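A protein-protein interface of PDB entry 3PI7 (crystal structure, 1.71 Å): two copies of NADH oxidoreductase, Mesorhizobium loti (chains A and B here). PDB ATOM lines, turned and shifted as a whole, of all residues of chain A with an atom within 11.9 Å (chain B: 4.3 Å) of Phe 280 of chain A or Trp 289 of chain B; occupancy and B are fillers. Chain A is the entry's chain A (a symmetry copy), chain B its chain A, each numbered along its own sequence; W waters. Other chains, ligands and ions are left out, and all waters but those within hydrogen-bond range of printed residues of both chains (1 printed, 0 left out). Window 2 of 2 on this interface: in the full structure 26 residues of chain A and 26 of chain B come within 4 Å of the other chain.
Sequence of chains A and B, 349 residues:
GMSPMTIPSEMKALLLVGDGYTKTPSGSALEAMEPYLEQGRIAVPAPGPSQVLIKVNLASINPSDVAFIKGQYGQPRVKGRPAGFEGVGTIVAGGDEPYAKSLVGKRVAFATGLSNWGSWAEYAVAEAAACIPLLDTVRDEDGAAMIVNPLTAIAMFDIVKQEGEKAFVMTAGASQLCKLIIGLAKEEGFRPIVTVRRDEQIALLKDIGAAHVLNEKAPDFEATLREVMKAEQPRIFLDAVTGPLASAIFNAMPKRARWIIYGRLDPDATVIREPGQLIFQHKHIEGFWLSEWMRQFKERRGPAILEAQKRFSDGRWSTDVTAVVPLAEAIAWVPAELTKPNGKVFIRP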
ATOM      1  N   PHE A 250     -16.683  -5.232 -27.488  1.00  0.00           N
ATOM      2  CA  PHE A 250     -17.476  -4.532 -26.503  1.00  0.00           C
ATOM      3  C   PHE A 250     -18.530  -5.440 -25.879  1.00  0.00           C
ATOM      4  O   PHE A 250     -18.682  -5.472 -24.660  1.00  0.00           O
ATOM      5  CB  PHE A 250     -18.140  -3.333 -27.163  1.00  0.00           C
ATOM      6  CG  PHE A 250     -18.960  -2.503 -26.206  1.00  0.00           C
ATOM      7  CD1 PHE A 250     -18.353  -1.841 -25.139  1.00  0.00           C
ATOM      8  CD2 PHE A 250     -20.327  -2.313 -26.419  1.00  0.00           C
ATOM      9  CE1 PHE A 250     -19.097  -1.022 -24.291  1.00  0.00           C
ATOM     10  CE2 PHE A 250     -21.069  -1.480 -25.582  1.00  0.00           C
ATOM     11  CZ  PHE A 250     -20.446  -0.838 -24.525  1.00  0.00           C
ATOM     12  N   ASN A 251     -19.239  -6.199 -26.714  1.00  0.00           N
ATOM     13  CA  ASN A 251     -20.271  -7.113 -26.254  1.00  0.00           C
ATOM     14  C   ASN A 251     -19.734  -8.155 -25.254  1.00  0.00           C
ATOM     15  O   ASN A 251     -20.419  -8.504 -24.287  1.00  0.00           O
ATOM     16  CB  ASN A 251     -20.857  -7.826 -27.468  1.00  0.00           C
ATOM     17  CG  ASN A 251     -22.055  -8.689 -27.159  1.00  0.00           C
ATOM     18  OD1 ASN A 251     -22.007  -9.919 -27.268  1.00  0.00           O
ATOM     19  ND2 ASN A 251     -23.120  -8.070 -26.730  1.00  0.00           N
ATOM     20  N   MET A 253     -17.046  -7.811 -23.320  1.00  0.00           N
ATOM     21  CA  MET A 253     -16.354  -7.278 -22.161  1.00  0.00           C
ATOM     22  C   MET A 253     -17.222  -7.305 -20.900  1.00  0.00           C
ATOM     23  O   MET A 253     -18.472  -7.333 -20.974  1.00  0.00           O
ATOM     24  CB  MET A 253     -15.836  -5.867 -22.438  1.00  0.00           C
ATOM     25  CG  MET A 253     -14.637  -5.862 -23.331  1.00  0.00           C
ATOM     26  SD  MET A 253     -14.311  -4.055 -23.833  1.00  0.00           S
ATOM     27  CE  MET A 253     -13.232  -3.497 -22.226  1.00  0.00           C
ATOM     28  N   PRO A 254     -16.564  -7.304 -19.705  1.00  0.00           N
ATOM     29  CA  PRO A 254     -17.344  -7.360 -18.468  1.00  0.00           C
ATOM     30  C   PRO A 254     -18.007  -6.026 -18.154  1.00  0.00           C
ATOM     31  O   PRO A 254     -17.858  -5.036 -18.892  1.00  0.00           O
ATOM     32  CB  PRO A 254     -16.294  -7.708 -17.407  1.00  0.00           C
ATOM     33  CG  PRO A 254     -15.051  -7.107 -17.903  1.00  0.00           C
ATOM     34  CD  PRO A 254     -15.104  -7.315 -19.406  1.00  0.00           C
ATOM     35  N   LYS A 255     -18.722  -6.003 -17.011  1.00  0.00           N
ATOM     36  CA  LYS A 255     -19.415  -4.812 -16.548  1.00  0.00           C
ATOM     37  C   LYS A 255     -18.438  -3.638 -16.356  1.00  0.00           C
ATOM     38  O   LYS A 255     -17.257  -3.818 -16.021  1.00  0.00           O
ATOM     39  CB  LYS A 255     -20.185  -5.093 -15.244  1.00  0.00           C
ATOM     40  CG  LYS A 255     -19.319  -5.459 -14.051  1.00  0.00           C
ATOM     41  CD  LYS A 255     -20.151  -5.986 -12.882  1.00  0.00           C
ATOM     42  CE  LYS A 255     -19.276  -6.606 -11.813  1.00  0.00           C
ATOM     43  N   ARG A 256     -18.957  -2.431 -16.603  1.00  0.00           N
ATOM     44  CA  ARG A 256     -18.282  -1.152 -16.451  1.00  0.00           C
ATOM     45  C   ARG A 256     -17.241  -0.921 -17.553  1.00  0.00           C
ATOM     46  O   ARG A 256     -16.439  -0.002 -17.443  1.00  0.00           O
ATOM     47  CB  ARG A 256     -17.659  -1.010 -15.054  1.00  0.00           C
ATOM     48  CG  ARG A 256     -18.680  -1.221 -13.950  1.00  0.00           C
ATOM     49  CD  ARG A 256     -18.249  -0.710 -12.596  1.00  0.00           C
ATOM     50  NE  ARG A 256     -19.355  -0.886 -11.644  1.00  0.00           N
ATOM     51  CZ  ARG A 256     -20.376  -0.041 -11.517  1.00  0.00           C
ATOM     52  NH1 ARG A 256     -20.432   1.064 -12.256  1.00  0.00           N
ATOM     53  NH2 ARG A 256     -21.354  -0.298 -10.658  1.00  0.00           N
ATOM     54  N   ALA A 257     -17.308  -1.701 -18.634  1.00  0.00           N
ATOM     55  CA  ALA A 257     -16.419  -1.535 -19.762  1.00  0.00           C
ATOM     56  C   ALA A 257     -16.632  -0.200 -20.437  1.00  0.00           C
ATOM     57  O   ALA A 257     -17.762   0.283 -20.525  1.00  0.00           O
ATOM     58  CB  ALA A 257     -16.635  -2.634 -20.763  1.00  0.00           C
ATOM     59  N   ILE A 272     -24.154  -1.479 -31.530  1.00  0.00           N
ATOM     60  CA  ILE A 272     -24.182  -1.765 -30.083  1.00  0.00           C
ATOM     61  C   ILE A 272     -25.067  -3.010 -30.036  1.00  0.00           C
ATOM     62  O   ILE A 272     -26.306  -2.906 -30.105  1.00  0.00           O
ATOM     63  CB  ILE A 272     -24.722  -0.597 -29.249  1.00  0.00           C
ATOM     64  CG1 ILE A 272     -23.933   0.704 -29.508  1.00  0.00           C
ATOM     65  CG2 ILE A 272     -24.707  -0.990 -27.766  1.00  0.00           C
ATOM     66  CD1 ILE A 272     -24.659   2.023 -29.016  1.00  0.00           C
ATOM     67  N   ARG A 273     -24.430  -4.190 -30.010  1.00  0.00           N
ATOM     68  CA  ARG A 273     -25.133  -5.464 -30.090  1.00  0.00           C
ATOM     69  C   ARG A 273     -26.219  -5.611 -29.027  1.00  0.00           C
ATOM     70  O   ARG A 273     -27.331  -6.028 -29.354  1.00  0.00           O
ATOM     71  CB  ARG A 273     -24.158  -6.643 -29.978  1.00  0.00           C
ATOM     72  CG  ARG A 273     -24.793  -7.949 -30.447  1.00  0.00           C
ATOM     73  CD  ARG A 273     -23.844  -9.120 -30.303  1.00  0.00           C
ATOM     74  NE  ARG A 273     -22.719  -9.040 -31.244  1.00  0.00           N
ATOM     75  CZ  ARG A 273     -21.746  -9.942 -31.316  1.00  0.00           C
ATOM     76  NH1 ARG A 273     -21.743 -10.989 -30.504  1.00  0.00           N
ATOM     77  NH2 ARG A 273     -20.761  -9.796 -32.195  1.00  0.00           N
ATOM     78  N   GLU A 274     -25.903  -5.275 -27.777  1.00  0.00           N
ATOM     79  CA  GLU A 274     -26.869  -5.413 -26.689  1.00  0.00           C
ATOM     80  C   GLU A 274     -26.926  -4.121 -25.914  1.00  0.00           C
ATOM     81  O   GLU A 274     -26.177  -3.967 -24.943  1.00  0.00           O
ATOM     82  CB  GLU A 274     -26.453  -6.573 -25.768  1.00  0.00           C
ATOM     83  CG  GLU A 274     -26.569  -7.966 -26.369  1.00  0.00           C
ATOM     84  CD  GLU A 274     -27.956  -8.419 -26.800  1.00  0.00           C
ATOM     85  OE1 GLU A 274     -28.949  -8.060 -26.124  1.00  0.00           O
ATOM     86  OE2 GLU A 274     -28.043  -9.152 -27.813  1.00  0.00           O
ATOM     87  N   PRO A 275     -27.755  -3.138 -26.330  1.00  0.00           N
ATOM     88  CA  PRO A 275     -27.796  -1.869 -25.590  1.00  0.00           C
ATOM     89  C   PRO A 275     -28.143  -2.037 -24.109  1.00  0.00           C
ATOM     90  O   PRO A 275     -27.722  -1.207 -23.307  1.00  0.00           O
ATOM     91  CB  PRO A 275     -28.882  -1.051 -26.323  1.00  0.00           C
ATOM     92  CG  PRO A 275     -28.871  -1.602 -27.693  1.00  0.00           C
ATOM     93  CD  PRO A 275     -28.667  -3.095 -27.487  1.00  0.00           C
ATOM     94  N   GLY A 276     -28.795  -3.154 -23.742  1.00  0.00           N
ATOM     95  CA  GLY A 276     -29.090  -3.481 -22.345  1.00  0.00           C
ATOM     96  C   GLY A 276     -27.828  -3.525 -21.493  1.00  0.00           C
ATOM     97  O   GLY A 276     -27.882  -3.287 -20.279  1.00  0.00           O
ATOM     98  N   GLN A 277     -26.662  -3.786 -22.125  1.00  0.00           N
ATOM     99  CA  GLN A 277     -25.391  -3.828 -21.382  1.00  0.00           C
ATOM    100  C   GLN A 277     -25.004  -2.446 -20.874  1.00  0.00           C
ATOM    101  O   GLN A 277     -24.314  -2.309 -19.885  1.00  0.00           O
ATOM    102  CB  GLN A 277     -24.274  -4.377 -22.248  1.00  0.00           C
ATOM    103  CG  GLN A 277     -24.525  -5.818 -22.576  1.00  0.00           C
ATOM    104  CD  GLN A 277     -23.387  -6.383 -23.361  1.00  0.00           C
ATOM    105  OE1 GLN A 277     -22.520  -5.661 -23.834  1.00  0.00           O
ATOM    106  NE2 GLN A 277     -23.376  -7.691 -23.497  1.00  0.00           N
ATOM    107  N   LEU A 278     -25.468  -1.418 -21.525  1.00  0.00           N
ATOM    108  CA  LEU A 278     -25.165  -0.081 -21.010  1.00  0.00           C
ATOM    109  C   LEU A 278     -26.048   0.167 -19.793  1.00  0.00           C
ATOM    110  O   LEU A 278     -25.619   0.807 -18.844  1.00  0.00           O
ATOM    111  CB  LEU A 278     -25.367   1.006 -22.064  1.00  0.00           C
ATOM    112  CG  LEU A 278     -24.332   0.979 -23.191  1.00  0.00           C
ATOM    113  CD1 LEU A 278     -24.954   0.457 -24.451  1.00  0.00           C
ATOM    114  CD2 LEU A 278     -23.716   2.329 -23.402  1.00  0.00           C
ATOM    115  N   ILE A 279     -27.272  -0.358 -19.814  1.00  0.00           N
ATOM    116  CA  ILE A 279     -28.207  -0.173 -18.683  1.00  0.00           C
ATOM    117  C   ILE A 279     -27.769  -0.980 -17.474  1.00  0.00           C
ATOM    118  O   ILE A 279     -27.459  -0.409 -16.431  1.00  0.00           O
ATOM    119  CB  ILE A 279     -29.646  -0.554 -19.073  1.00  0.00           C
ATOM    120  CG1 ILE A 279     -30.134   0.219 -20.319  1.00  0.00           C
ATOM    121  CG2 ILE A 279     -30.616  -0.474 -17.866  1.00  0.00           C
ATOM    122  CD1 ILE A 279     -31.415  -0.344 -20.939  1.00  0.00           C
ATOM    123  N   PHE A 280     -27.726  -2.311 -17.637  1.00  0.00           N
ATOM    124  CA  PHE A 280     -27.506  -3.288 -16.584  1.00  0.00           C
ATOM    125  C   PHE A 280     -26.048  -3.579 -16.249  1.00  0.00           C
ATOM    126  O   PHE A 280     -25.780  -3.981 -15.114  1.00  0.00           O
ATOM    127  CB  PHE A 280     -28.230  -4.608 -16.959  1.00  0.00           C
ATOM    128  CG  PHE A 280     -29.711  -4.357 -17.134  1.00  0.00           C
ATOM    129  CD1 PHE A 280     -30.503  -3.973 -16.052  1.00  0.00           C
ATOM    130  CD2 PHE A 280     -30.299  -4.418 -18.392  1.00  0.00           C
ATOM    131  CE1 PHE A 280     -31.868  -3.691 -16.224  1.00  0.00           C
ATOM    132  CE2 PHE A 280     -31.664  -4.114 -18.567  1.00  0.00           C
ATOM    133  CZ  PHE A 280     -32.428  -3.733 -17.488  1.00  0.00           C
ATOM    134  N   GLN A 281     -25.118  -3.382 -17.194  1.00  0.00           N
ATOM    135  CA  GLN A 281     -23.707  -3.665 -16.939  1.00  0.00           C
ATOM    136  C   GLN A 281     -22.881  -2.373 -16.903  1.00  0.00           C
ATOM    137  O   GLN A 281     -21.664  -2.421 -16.813  1.00  0.00           O
ATOM    138  CB  GLN A 281     -23.160  -4.672 -17.953  1.00  0.00           C
ATOM    139  CG  GLN A 281     -23.895  -6.018 -17.892  1.00  0.00           C
ATOM    140  CD  GLN A 281     -23.322  -7.059 -18.828  1.00  0.00           C
ATOM    141  OE1 GLN A 281     -22.494  -6.776 -19.694  1.00  0.00           O
ATOM    142  NE2 GLN A 281     -23.785  -8.292 -18.694  1.00  0.00           N
ATOM    143  N   HIS A 282     -23.558  -1.215 -16.897  1.00  0.00           N
ATOM    144  CA  HIS A 282     -22.935   0.105 -16.715  1.00  0.00           C
ATOM    145  C   HIS A 282     -21.820   0.394 -17.724  1.00  0.00           C
ATOM    146  O   HIS A 282     -20.835   1.064 -17.387  1.00  0.00           O
ATOM    147  CB  HIS A 282     -22.378   0.234 -15.269  1.00  0.00           C
ATOM    148  CG  HIS A 282     -23.133  -0.587 -14.252  1.00  0.00           C
ATOM    149  ND1 HIS A 282     -24.461  -0.310 -13.930  1.00  0.00           N
ATOM    150  CD2 HIS A 282     -22.747  -1.705 -13.584  1.00  0.00           C
ATOM    151  CE1 HIS A 282     -24.825  -1.241 -13.060  1.00  0.00           C
ATOM    152  NE2 HIS A 282     -23.815  -2.093 -12.799  1.00  0.00           N
ATOM    153  N   LYS A 283     -21.967  -0.112 -18.946  1.00  0.00           N
ATOM    154  CA  LYS A 283     -20.947   0.088 -19.991  1.00  0.00           C
ATOM    155  C   LYS A 283     -21.088   1.490 -20.579  1.00  0.00           C
ATOM    156  O   LYS A 283     -22.160   2.094 -20.479  1.00  0.00           O
ATOM    157  CB  LYS A 283     -21.045  -0.982 -21.096  1.00  0.00           C
ATOM    158  CG  LYS A 283     -20.660  -2.379 -20.623  1.00  0.00           C
ATOM    159  CD  LYS A 283     -20.572  -3.347 -21.793  1.00  0.00           C
ATOM    160  CE  LYS A 283     -20.235  -4.722 -21.257  1.00  0.00           C
ATOM    161  NZ  LYS A 283     -20.201  -5.735 -22.377  1.00  0.00           N
ATOM    162  N   HIS A 284     -19.973   2.043 -21.100  1.00  0.00           N
ATOM    163  CA  HIS A 284     -19.936   3.389 -21.662  1.00  0.00           C
ATOM    164  C   HIS A 284     -19.257   3.362 -22.996  1.00  0.00           C
ATOM    165  O   HIS A 284     -18.390   2.521 -23.238  1.00  0.00           O
ATOM    166  CB  HIS A 284     -19.135   4.333 -20.741  1.00  0.00           C
ATOM    167  CG  HIS A 284     -19.928   4.926 -19.641  1.00  0.00           C
ATOM    168  ND1 HIS A 284     -20.210   4.205 -18.478  1.00  0.00           N
ATOM    169  CD2 HIS A 284     -20.490   6.150 -19.550  1.00  0.00           C
ATOM    170  CE1 HIS A 284     -20.962   5.007 -17.727  1.00  0.00           C
ATOM    171  NE2 HIS A 284     -21.162   6.184 -18.322  1.00  0.00           N
ATOM    172  N   TYR B  73     -35.420  -8.748 -19.687  1.00  0.00           N
ATOM    173  CA  TYR B  73     -35.001  -7.691 -18.779  1.00  0.00           C
ATOM    174  C   TYR B  73     -33.621  -8.029 -18.177  1.00  0.00           C
ATOM    175  O   TYR B  73     -33.083  -9.093 -18.440  1.00  0.00           O
ATOM    176  CB  TYR B  73     -36.075  -7.507 -17.680  1.00  0.00           C
ATOM    177  CG  TYR B  73     -35.902  -6.246 -16.865  1.00  0.00           C
ATOM    178  CD1 TYR B  73     -36.046  -4.990 -17.451  1.00  0.00           C
ATOM    179  CD2 TYR B  73     -35.698  -6.307 -15.489  1.00  0.00           C
ATOM    180  CE1 TYR B  73     -35.907  -3.825 -16.702  1.00  0.00           C
ATOM    181  CE2 TYR B  73     -35.545  -5.144 -14.731  1.00  0.00           C
ATOM    182  CZ  TYR B  73     -35.671  -3.905 -15.341  1.00  0.00           C
ATOM    183  OH  TYR B  73     -35.516  -2.746 -14.621  1.00  0.00           O
ATOM    184  N   GLY B  74     -33.041  -7.115 -17.419  1.00  0.00           N
ATOM    185  CA  GLY B  74     -31.740  -7.329 -16.801  1.00  0.00           C
ATOM    186  C   GLY B  74     -31.800  -8.052 -15.478  1.00  0.00           C
ATOM    187  O   GLY B  74     -30.880  -7.934 -14.670  1.00  0.00           O
ATOM    188  N   PHE B 288     -28.729   4.249 -18.190  1.00  0.00           N
ATOM    189  CA  PHE B 288     -29.265   4.674 -16.923  1.00  0.00           C
ATOM    190  C   PHE B 288     -30.110   3.534 -16.398  1.00  0.00           C
ATOM    191  O   PHE B 288     -30.974   3.047 -17.125  1.00  0.00           O
ATOM    192  CB  PHE B 288     -30.119   5.960 -17.061  1.00  0.00           C
ATOM    193  CG  PHE B 288     -30.700   6.333 -15.721  1.00  0.00           C
ATOM    194  CD1 PHE B 288     -31.921   5.804 -15.301  1.00  0.00           C
ATOM    195  CD2 PHE B 288     -30.001   7.161 -14.851  1.00  0.00           C
ATOM    196  CE1 PHE B 288     -32.445   6.129 -14.051  1.00  0.00           C
ATOM    197  CE2 PHE B 288     -30.529   7.476 -13.588  1.00  0.00           C
ATOM    198  CZ  PHE B 288     -31.728   6.930 -13.194  1.00  0.00           C
ATOM    199  N   TRP B 289     -29.929   3.200 -15.116  1.00  0.00           N
ATOM    200  CA  TRP B 289     -30.677   2.161 -14.436  1.00  0.00           C
ATOM    201  C   TRP B 289     -31.027   2.680 -13.057  1.00  0.00           C
ATOM    202  O   TRP B 289     -30.135   3.034 -12.298  1.00  0.00           O
ATOM    203  CB  TRP B 289     -29.837   0.885 -14.371  1.00  0.00           C
ATOM    204  CG  TRP B 289     -30.523  -0.317 -13.797  1.00  0.00           C
ATOM    205  CD1 TRP B 289     -31.862  -0.538 -13.670  1.00  0.00           C
ATOM    206  CD2 TRP B 289     -29.871  -1.498 -13.329  1.00  0.00           C
ATOM    207  NE1 TRP B 289     -32.082  -1.775 -13.098  1.00  0.00           N
ATOM    208  CE2 TRP B 289     -30.871  -2.371 -12.848  1.00  0.00           C
ATOM    209  CE3 TRP B 289     -28.527  -1.877 -13.207  1.00  0.00           C
ATOM    210  CZ2 TRP B 289     -30.572  -3.643 -12.345  1.00  0.00           C
ATOM    211  CZ3 TRP B 289     -28.228  -3.133 -12.702  1.00  0.00           C
ATOM    212  CH2 TRP B 289     -29.243  -3.995 -12.268  1.00  0.00           C
ATOM    213  N   LEU B 290     -32.329   2.835 -12.785  1.00  0.00           N
ATOM    214  CA  LEU B 290     -32.747   3.415 -11.490  1.00  0.00           C
ATOM    215  C   LEU B 290     -32.154   2.649 -10.299  1.00  0.00           C
ATOM    216  O   LEU B 290     -31.631   3.288  -9.383  1.00  0.00           O
ATOM    217  CB  LEU B 290     -34.269   3.476 -11.406  1.00  0.00           C
ATOM    218  CG  LEU B 290     -34.841   4.038 -10.084  1.00  0.00           C
ATOM    219  CD1 LEU B 290     -34.432   5.505  -9.836  1.00  0.00           C
ATOM    220  CD2 LEU B 290     -36.302   3.798 -10.010  1.00  0.00           C
ATOM    221  N   SER B 291     -32.143   1.298 -10.351  1.00  0.00           N
ATOM    222  CA  SER B 291     -31.554   0.507  -9.252  1.00  0.00           C
ATOM    223  C   SER B 291     -30.097   0.880  -9.026  1.00  0.00           C
ATOM    224  O   SER B 291     -29.693   1.040  -7.872  1.00  0.00           O
ATOM    225  CB  SER B 291     -31.686  -0.993  -9.499  1.00  0.00           C
ATOM    226  OG  SER B 291     -33.048  -1.369  -9.631  1.00  0.00           O
ATOM    227  N   GLU B 292     -29.316   1.106 -10.118  1.00  0.00           N
ATOM    228  CA  GLU B 292     -27.930   1.511  -9.989  1.00  0.00           C
ATOM    229  C   GLU B 292     -27.796   2.919  -9.448  1.00  0.00           C
ATOM    230  O   GLU B 292     -26.965   3.140  -8.580  1.00  0.00           O
ATOM    231  CB  GLU B 292     -27.163   1.374 -11.328  1.00  0.00           C
ATOM    232  CG  GLU B 292     -25.672   1.650 -11.202  1.00  0.00           C
ATOM    233  CD  GLU B 292     -24.822   0.802 -10.266  1.00  0.00           C
ATOM    234  OE1 GLU B 292     -25.299  -0.255  -9.786  1.00  0.00           O
ATOM    235  OE2 GLU B 292     -23.650   1.187 -10.047  1.00  0.00           O
ATOM    236  N   TRP B 293     -28.646   3.857  -9.911  1.00  0.00           N
ATOM    237  CA  TRP B 293     -28.618   5.236  -9.467  1.00  0.00           C
ATOM    238  C   TRP B 293     -28.847   5.293  -7.941  1.00  0.00           C
ATOM    239  O   TRP B 293     -28.144   6.023  -7.265  1.00  0.00           O
ATOM    240  CB  TRP B 293     -29.670   6.054 -10.229  1.00  0.00           C
ATOM    241  CG  TRP B 293     -29.734   7.495  -9.817  1.00  0.00           C
ATOM    242  CD1 TRP B 293     -28.995   8.530 -10.307  1.00  0.00           C
ATOM    243  CD2 TRP B 293     -30.574   8.048  -8.800  1.00  0.00           C
ATOM    244  NE1 TRP B 293     -29.343   9.704  -9.670  1.00  0.00           N
ATOM    245  CE2 TRP B 293     -30.300   9.433  -8.733  1.00  0.00           C
ATOM    246  CE3 TRP B 293     -31.594   7.520  -7.996  1.00  0.00           C
ATOM    247  CZ2 TRP B 293     -30.984  10.288  -7.862  1.00  0.00           C
ATOM    248  CZ3 TRP B 293     -32.224   8.359  -7.086  1.00  0.00           C
ATOM    249  CH2 TRP B 293     -31.909   9.723  -7.022  1.00  0.00           C
ATOM    250  N   ARG B 295     -28.196   2.941  -5.772  1.00  0.00           N
ATOM    251  CA  ARG B 295     -27.006   2.362  -5.140  1.00  0.00           C
ATOM    252  C   ARG B 295     -25.872   3.375  -5.090  1.00  0.00           C
ATOM    253  O   ARG B 295     -25.231   3.537  -4.051  1.00  0.00           O
ATOM    254  CB  ARG B 295     -26.532   1.105  -5.886  1.00  0.00           C
ATOM    255  CG  ARG B 295     -27.282  -0.160  -5.513  1.00  0.00           C
ATOM    256  CD  ARG B 295     -26.614  -1.401  -6.077  1.00  0.00           C
ATOM    257  NE  ARG B 295     -26.759  -1.485  -7.530  1.00  0.00           N
ATOM    258  CZ  ARG B 295     -27.704  -2.181  -8.155  1.00  0.00           C
ATOM    259  NH1 ARG B 295     -28.597  -2.878  -7.461  1.00  0.00           N
ATOM    260  NH2 ARG B 295     -27.759  -2.190  -9.479  1.00  0.00           N
HETATM  261  O   HOH W   1     -22.658   3.022 -11.815  1.00  0.00           O
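The guanidinium group (NH2) of Arg 256 of chain A is in salt-bridge range of the side-chain carboxylate (OE2) of Glu 292 of chain B, at 2.8 Å.
The guanidinium group (NE) of Arg 295 of chain B is in salt-bridge range of the side-chain carboxylate (OE1) of Glu 292 of chain B (3.0 Å).
The backbone carbonyl oxygen (O) of Gln 281 of chain A lies within hydrogen-bond range of the backbone NH (N) of Arg 256 of chain A.
The backbone NH of His 282 of chain A sits at hydrogen-bond distance from the backbone carbonyl oxygen of Gln 277 of chain A, 3.3 Å away.
The backbone carbonyl oxygen of His 282 of chain A sits at hydrogen-bond distance from a ring nitrogen (ND1) of His 284 of chain A (3.4 Å).
Pro 254 of chain A touches none of the printed residues of chain B.
Printed residues of chain B within 4 Å of Arg 256 of chain A: Glu 292.
Printed residues of chain B within 4 Å of Ile 279 of chain A: Phe 288 (3.6 Å) and Trp 289 (3.4 Å).
Of chain B, only Tyr 73, Gly 74 and Trp 289 come within 4 Å of Phe 280 of chain A.
Gln 281 of chain A touches none of the printed residues of chain B.
Of the printed residues of chain B, His 282 of chain A touches Trp 289 (3.8 Å) and Glu 292 (3.5 Å).
Printed residues of chain A within 4 Å of Tyr 73 of chain B: Phe 280.
Trp 289 of chain B touches three residues of chain A.
No residue of chain A comes within 4 Å of Leu 290 of chain B.
No residue of chain A comes within 4 Å of Ser 291 of chain B.
Glu 292 of chain B touches just these residues of chain A: Arg 256 (2.8 Å) and His 282 (3.5 Å).
The nearest printed residue of chain B that does not touch Phe 280 of chain A is Arg 295 of chain B (6.2 Å).
The nearest printed residue of chain A that does not touch Trp 289 of chain B is Gln 281 of chain A (5.5 Å).
The nearest printed residue of chain B that does not touch Arg 256 of chain A is Arg 295 of chain B (6.4 Å).
Printed residues of chain B that touch a printed residue of chain A: Tyr 73, Gly 74, Phe 288, Trp 289 and Glu 292.
Of the 20 printed residues of chain A, 4 touch a printed residue of chain B.
Among the printed residues, Asp or Glu carboxylates within 4 Å of a Lys or Arg side-chain nitrogen of the other chain: Arg 256 of chain A with Glu 292 of chain B (2.8 Å).
Among the printed residues, merely in contact across the chains: Ile 279 of chain A with Phe 288 of chain B, Ile 279 of chain A with Trp 289 of chain B, Phe 280 of chain A with Tyr 73 of chain B, Phe 280 of chain A with Gly 74 of chain B, Phe 280 of chain A with Trp 289 of chain B, His 282 of chain A with Trp 289 of chain B and His 282 of chain A with Glu 292 of chain B.
No position is printed for both chains.
Of the 8 pairs that touch across the chains among the printed residues, none has its exchanged pair printed and touching as well.
Water W1 lies within hydrogen-bond range of the side-chain carboxylate of Glu 292 of chain B (2.7 Å) and the guanidinium group of Arg 256 of chain A (3.0 Å).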
